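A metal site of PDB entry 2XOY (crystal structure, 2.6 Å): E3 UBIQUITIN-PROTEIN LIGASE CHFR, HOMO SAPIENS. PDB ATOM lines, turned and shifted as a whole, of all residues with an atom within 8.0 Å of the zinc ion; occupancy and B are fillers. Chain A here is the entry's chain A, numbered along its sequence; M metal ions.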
ATOM      1  N   THR A  83     -13.228   3.763   7.319  1.00  0.00           N
ATOM      2  CA  THR A  83     -12.901   5.143   7.610  1.00  0.00           C
ATOM      3  C   THR A  83     -13.911   6.098   6.978  1.00  0.00           C
ATOM      4  O   THR A  83     -14.045   7.233   7.412  1.00  0.00           O
ATOM      5  CB  THR A  83     -11.503   5.464   7.083  1.00  0.00           C
ATOM      6  OG1 THR A  83     -10.554   4.602   7.734  1.00  0.00           O
ATOM      7  CG2 THR A  83     -11.149   6.945   7.307  1.00  0.00           C
ATOM      8  N   GLN A 106      -7.599  -1.736   3.161  1.00  0.00           N
ATOM      9  CA  GLN A 106      -6.931  -0.511   3.556  1.00  0.00           C
ATOM     10  C   GLN A 106      -6.236   0.235   2.418  1.00  0.00           C
ATOM     11  O   GLN A 106      -5.794  -0.361   1.444  1.00  0.00           O
ATOM     12  CB  GLN A 106      -5.937  -0.778   4.695  1.00  0.00           C
ATOM     13  CG  GLN A 106      -4.745  -1.649   4.321  1.00  0.00           C
ATOM     14  CD  GLN A 106      -3.711  -1.695   5.427  1.00  0.00           C
ATOM     15  OE1 GLN A 106      -4.030  -2.017   6.571  1.00  0.00           O
ATOM     16  NE2 GLN A 106      -2.487  -1.351   5.094  1.00  0.00           N
ATOM     17  N   CYS A 107      -6.166   1.550   2.558  1.00  0.00           N
ATOM     18  CA  CYS A 107      -5.399   2.350   1.640  1.00  0.00           C
ATOM     19  C   CYS A 107      -3.897   2.081   1.815  1.00  0.00           C
ATOM     20  O   CYS A 107      -3.380   2.001   2.919  1.00  0.00           O
ATOM     21  CB  CYS A 107      -5.705   3.827   1.858  1.00  0.00           C
ATOM     22  SG  CYS A 107      -4.677   4.848   0.852  1.00  0.00           S
ATOM     23  N   ALA A 108      -3.186   1.929   0.702  1.00  0.00           N
ATOM     24  CA  ALA A 108      -1.788   1.555   0.811  1.00  0.00           C
ATOM     25  C   ALA A 108      -0.900   2.754   0.979  1.00  0.00           C
ATOM     26  O   ALA A 108       0.312   2.655   0.853  1.00  0.00           O
ATOM     27  CB  ALA A 108      -1.358   0.735  -0.371  1.00  0.00           C
ATOM     28  N   VAL A 109      -1.496   3.900   1.274  1.00  0.00           N
ATOM     29  CA  VAL A 109      -0.715   5.116   1.493  1.00  0.00           C
ATOM     30  C   VAL A 109      -0.902   5.630   2.909  1.00  0.00           C
ATOM     31  O   VAL A 109       0.060   5.813   3.647  1.00  0.00           O
ATOM     32  CB  VAL A 109      -1.089   6.216   0.483  1.00  0.00           C
ATOM     33  CG1 VAL A 109      -0.239   7.471   0.710  1.00  0.00           C
ATOM     34  CG2 VAL A 109      -0.912   5.700  -0.943  1.00  0.00           C
ATOM     35  N   CYS A 110      -2.147   5.873   3.296  1.00  0.00           N
ATOM     36  CA  CYS A 110      -2.434   6.353   4.645  1.00  0.00           C
ATOM     37  C   CYS A 110      -2.504   5.152   5.609  1.00  0.00           C
ATOM     38  O   CYS A 110      -2.281   5.292   6.802  1.00  0.00           O
ATOM     39  CB  CYS A 110      -3.715   7.180   4.668  1.00  0.00           C
ATOM     40  SG  CYS A 110      -5.203   6.268   4.188  1.00  0.00           S
ATOM     41  N   LEU A 111      -2.807   3.988   5.055  1.00  0.00           N
ATOM     42  CA  LEU A 111      -2.872   2.733   5.796  1.00  0.00           C
ATOM     43  C   LEU A 111      -4.140   2.593   6.658  1.00  0.00           C
ATOM     44  O   LEU A 111      -4.263   1.650   7.448  1.00  0.00           O
ATOM     45  CB  LEU A 111      -1.597   2.516   6.622  1.00  0.00           C
ATOM     46  CG  LEU A 111      -0.299   2.545   5.831  1.00  0.00           C
ATOM     47  CD1 LEU A 111       0.908   2.427   6.752  1.00  0.00           C
ATOM     48  CD2 LEU A 111      -0.288   1.464   4.753  1.00  0.00           C
ATOM     49  N   GLN A 112      -5.070   3.521   6.483  1.00  0.00           N
ATOM     50  CA  GLN A 112      -6.387   3.431   7.112  1.00  0.00           C
ATOM     51  C   GLN A 112      -7.298   2.421   6.406  1.00  0.00           C
ATOM     52  O   GLN A 112      -7.058   2.076   5.254  1.00  0.00           O
ATOM     53  CB  GLN A 112      -7.034   4.817   7.145  1.00  0.00           C
ATOM     54  CG  GLN A 112      -6.199   5.846   7.902  1.00  0.00           C
ATOM     55  CD  GLN A 112      -5.616   5.290   9.211  1.00  0.00           C
ATOM     56  OE1 GLN A 112      -6.350   4.785  10.065  1.00  0.00           O
ATOM     57  NE2 GLN A 112      -4.282   5.374   9.360  1.00  0.00           N
ATOM     58  N   PRO A 113      -8.334   1.934   7.105  1.00  0.00           N
ATOM     59  CA  PRO A 113      -9.174   0.859   6.565  1.00  0.00           C
ATOM     60  C   PRO A 113     -10.443   1.374   5.885  1.00  0.00           C
ATOM     61  O   PRO A 113     -11.023   2.383   6.317  1.00  0.00           O
ATOM     62  CB  PRO A 113      -9.567   0.071   7.830  1.00  0.00           C
ATOM     63  CG  PRO A 113      -9.054   0.898   9.005  1.00  0.00           C
ATOM     64  CD  PRO A 113      -8.713   2.240   8.483  1.00  0.00           C
ATOM     65  N   PHE A 114     -10.869   0.658   4.841  1.00  0.00           N
ATOM     66  CA  PHE A 114     -12.030   1.062   4.051  1.00  0.00           C
ATOM     67  C   PHE A 114     -12.744  -0.164   3.554  1.00  0.00           C
ATOM     68  O   PHE A 114     -12.105  -1.144   3.189  1.00  0.00           O
ATOM     69  CB  PHE A 114     -11.577   1.903   2.849  1.00  0.00           C
ATOM     70  CG  PHE A 114     -10.986   3.236   3.227  1.00  0.00           C
ATOM     71  CD1 PHE A 114     -11.788   4.366   3.279  1.00  0.00           C
ATOM     72  CD2 PHE A 114      -9.644   3.356   3.531  1.00  0.00           C
ATOM     73  CE1 PHE A 114     -11.268   5.593   3.609  1.00  0.00           C
ATOM     74  CE2 PHE A 114      -9.116   4.586   3.862  1.00  0.00           C
ATOM     75  CZ  PHE A 114      -9.936   5.711   3.903  1.00  0.00           C
ATOM     76  N   CYS A 129     -14.844   4.457  -2.139  1.00  0.00           N
ATOM     77  CA  CYS A 129     -13.722   4.976  -1.345  1.00  0.00           C
ATOM     78  C   CYS A 129     -12.420   4.186  -1.422  1.00  0.00           C
ATOM     79  O   CYS A 129     -11.455   4.525  -0.743  1.00  0.00           O
ATOM     80  CB  CYS A 129     -14.141   5.181   0.120  1.00  0.00           C
ATOM     81  SG  CYS A 129     -15.001   3.770   0.901  1.00  0.00           S
ATOM     82  N   LEU A 130     -12.380   3.124  -2.225  1.00  0.00           N
ATOM     83  CA  LEU A 130     -11.134   2.380  -2.421  1.00  0.00           C
ATOM     84  C   LEU A 130     -11.058   1.763  -3.808  1.00  0.00           C
ATOM     85  O   LEU A 130     -11.984   1.085  -4.252  1.00  0.00           O
ATOM     86  CB  LEU A 130     -10.933   1.316  -1.329  1.00  0.00           C
ATOM     87  CG  LEU A 130      -9.511   0.809  -1.051  1.00  0.00           C
ATOM     88  CD1 LEU A 130      -8.696   1.823  -0.235  1.00  0.00           C
ATOM     89  CD2 LEU A 130      -9.510  -0.571  -0.360  1.00  0.00           C
ATOM     90  N   ASP A 188       4.056  11.483  -2.674  1.00  0.00           N
ATOM     91  CA  ASP A 188       4.015  10.072  -2.313  1.00  0.00           C
ATOM     92  C   ASP A 188       4.657   9.364  -3.485  1.00  0.00           C
ATOM     93  O   ASP A 188       3.987   8.813  -4.344  1.00  0.00           O
ATOM     94  CB  ASP A 188       2.572   9.618  -2.082  1.00  0.00           C
ATOM     95  CG  ASP A 188       1.860  10.456  -1.025  1.00  0.00           C
ATOM     96  OD1 ASP A 188       2.513  10.845  -0.034  1.00  0.00           O
ATOM     97  OD2 ASP A 188       0.647  10.732  -1.182  1.00  0.00           O
ATOM     98  N   VAL A 196      -3.507   0.572  -4.745  1.00  0.00           N
ATOM     99  CA  VAL A 196      -4.820   0.503  -4.141  1.00  0.00           C
ATOM    100  C   VAL A 196      -4.913   1.574  -3.072  1.00  0.00           C
ATOM    101  O   VAL A 196      -4.290   1.457  -2.026  1.00  0.00           O
ATOM    102  CB  VAL A 196      -5.076  -0.872  -3.539  1.00  0.00           C
ATOM    103  CG1 VAL A 196      -6.256  -0.820  -2.586  1.00  0.00           C
ATOM    104  CG2 VAL A 196      -5.312  -1.903  -4.652  1.00  0.00           C
ATOM    105  N   LEU A 197      -5.672   2.624  -3.326  1.00  0.00           N
ATOM    106  CA  LEU A 197      -5.714   3.718  -2.368  1.00  0.00           C
ATOM    107  C   LEU A 197      -7.083   4.338  -2.169  1.00  0.00           C
ATOM    108  O   LEU A 197      -8.061   3.945  -2.800  1.00  0.00           O
ATOM    109  CB  LEU A 197      -4.666   4.769  -2.710  1.00  0.00           C
ATOM    110  CG  LEU A 197      -4.644   5.275  -4.139  1.00  0.00           C
ATOM    111  CD1 LEU A 197      -6.013   5.822  -4.471  1.00  0.00           C
ATOM    112  CD2 LEU A 197      -3.574   6.349  -4.299  1.00  0.00           C
ATOM    113  N   CYS A 198      -7.148   5.322  -1.293  1.00  0.00           N
ATOM    114  CA  CYS A 198      -8.422   5.892  -0.906  1.00  0.00           C
ATOM    115  C   CYS A 198      -8.758   7.216  -1.594  1.00  0.00           C
ATOM    116  O   CYS A 198      -7.914   7.842  -2.243  1.00  0.00           O
ATOM    117  CB  CYS A 198      -8.540   6.019   0.615  1.00  0.00           C
ATOM    118  SG  CYS A 198      -7.558   7.324   1.348  1.00  0.00           S
ATOM    119  N   TYR A 199     -10.011   7.619  -1.443  1.00  0.00           N
ATOM    120  CA  TYR A 199     -10.487   8.826  -2.063  1.00  0.00           C
ATOM    121  C   TYR A 199      -9.533   9.975  -1.747  1.00  0.00           C
ATOM    122  O   TYR A 199      -9.077  10.663  -2.670  1.00  0.00           O
ATOM    123  CB  TYR A 199     -11.935   9.159  -1.629  1.00  0.00           C
ATOM    124  CG  TYR A 199     -12.323  10.581  -1.975  1.00  0.00           C
ATOM    125  CD1 TYR A 199     -12.595  10.965  -3.277  1.00  0.00           C
ATOM    126  CD2 TYR A 199     -12.413  11.553  -0.986  1.00  0.00           C
ATOM    127  CE1 TYR A 199     -12.934  12.262  -3.588  1.00  0.00           C
ATOM    128  CE2 TYR A 199     -12.755  12.856  -1.284  1.00  0.00           C
ATOM    129  CZ  TYR A 199     -13.002  13.206  -2.587  1.00  0.00           C
ATOM    130  OH  TYR A 199     -13.344  14.512  -2.895  1.00  0.00           O
ATOM    131  N   CYS A 200      -9.197  10.172  -0.471  1.00  0.00           N
ATOM    132  CA  CYS A 200      -8.421  11.346  -0.086  1.00  0.00           C
ATOM    133  C   CYS A 200      -6.982  11.310  -0.612  1.00  0.00           C
ATOM    134  O   CYS A 200      -6.435  12.325  -1.030  1.00  0.00           O
ATOM    135  CB  CYS A 200      -8.472  11.572   1.428  1.00  0.00           C
ATOM    136  SG  CYS A 200     -10.031  12.353   2.015  1.00  0.00           S
ATOM    137  N   CYS A 201      -6.390  10.127  -0.606  1.00  0.00           N
ATOM    138  CA  CYS A 201      -5.016   9.997  -1.030  1.00  0.00           C
ATOM    139  C   CYS A 201      -4.929  10.149  -2.542  1.00  0.00           C
ATOM    140  O   CYS A 201      -4.088  10.891  -3.054  1.00  0.00           O
ATOM    141  CB  CYS A 201      -4.403   8.662  -0.536  1.00  0.00           C
ATOM    142  SG  CYS A 201      -4.132   8.619   1.279  1.00  0.00           S
ATOM    143  N   GLY A 202      -5.811   9.462  -3.262  1.00  0.00           N
ATOM    144  CA  GLY A 202      -5.873   9.597  -4.708  1.00  0.00           C
ATOM    145  C   GLY A 202      -6.090  11.038  -5.131  1.00  0.00           C
ATOM    146  O   GLY A 202      -5.406  11.563  -6.008  1.00  0.00           O
ATOM    147  N   ARG A 204      -5.387  13.797  -3.438  1.00  0.00           N
ATOM    148  CA  ARG A 204      -4.167  14.531  -3.203  1.00  0.00           C
ATOM    149  C   ARG A 204      -3.173  14.382  -4.361  1.00  0.00           C
ATOM    150  O   ARG A 204      -2.628  15.362  -4.852  1.00  0.00           O
ATOM    151  CB  ARG A 204      -3.526  14.117  -1.867  1.00  0.00           C
ATOM    152  CG  ARG A 204      -2.239  14.865  -1.579  1.00  0.00           C
ATOM    153  CD  ARG A 204      -1.662  14.524  -0.240  1.00  0.00           C
ATOM    154  NE  ARG A 204      -1.484  13.088  -0.074  1.00  0.00           N
ATOM    155  CZ  ARG A 204      -2.185  12.349   0.775  1.00  0.00           C
ATOM    156  NH1 ARG A 204      -3.114  12.921   1.539  1.00  0.00           N
ATOM    157  NH2 ARG A 204      -1.958  11.039   0.859  1.00  0.00           N
HETATM  158 ZN    ZN M   1      -5.393   6.939   1.922  1.00  0.00          ZN
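SG of Cys 201 lies close to NH2 of Arg 204 (3.3 Å).
SG of Cys 198 sits close to N of Cys 200 (3.8 Å).
The side-chain amide nitrogen (NE2) of Gln 112 lies within hydrogen-bond range of the backbone carbonyl oxygen (O) of Cys 110, 3.2 Å away.
The backbone NH (N) of Val 109 lies close to the side-chain sulfur (SG) of Cys 107, 3.3 Å away.
The backbone carbonyl oxygen (O) of Gln 112 is in hydrogen-bond range of the backbone NH (N) of Cys 107, at 2.9 Å.
The zinc ion is bound by the side-chain sulfur (SG) of Cys 201 (2.2 Å), the side-chain sulfur (SG) of Cys 198 (2.3 Å), the side-chain sulfur (SG) of Cys 110 (2.4 Å) and the side-chain sulfur (SG) of Cys 107 (2.5 Å).
The zinc ion has four donor atoms within binding distance.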
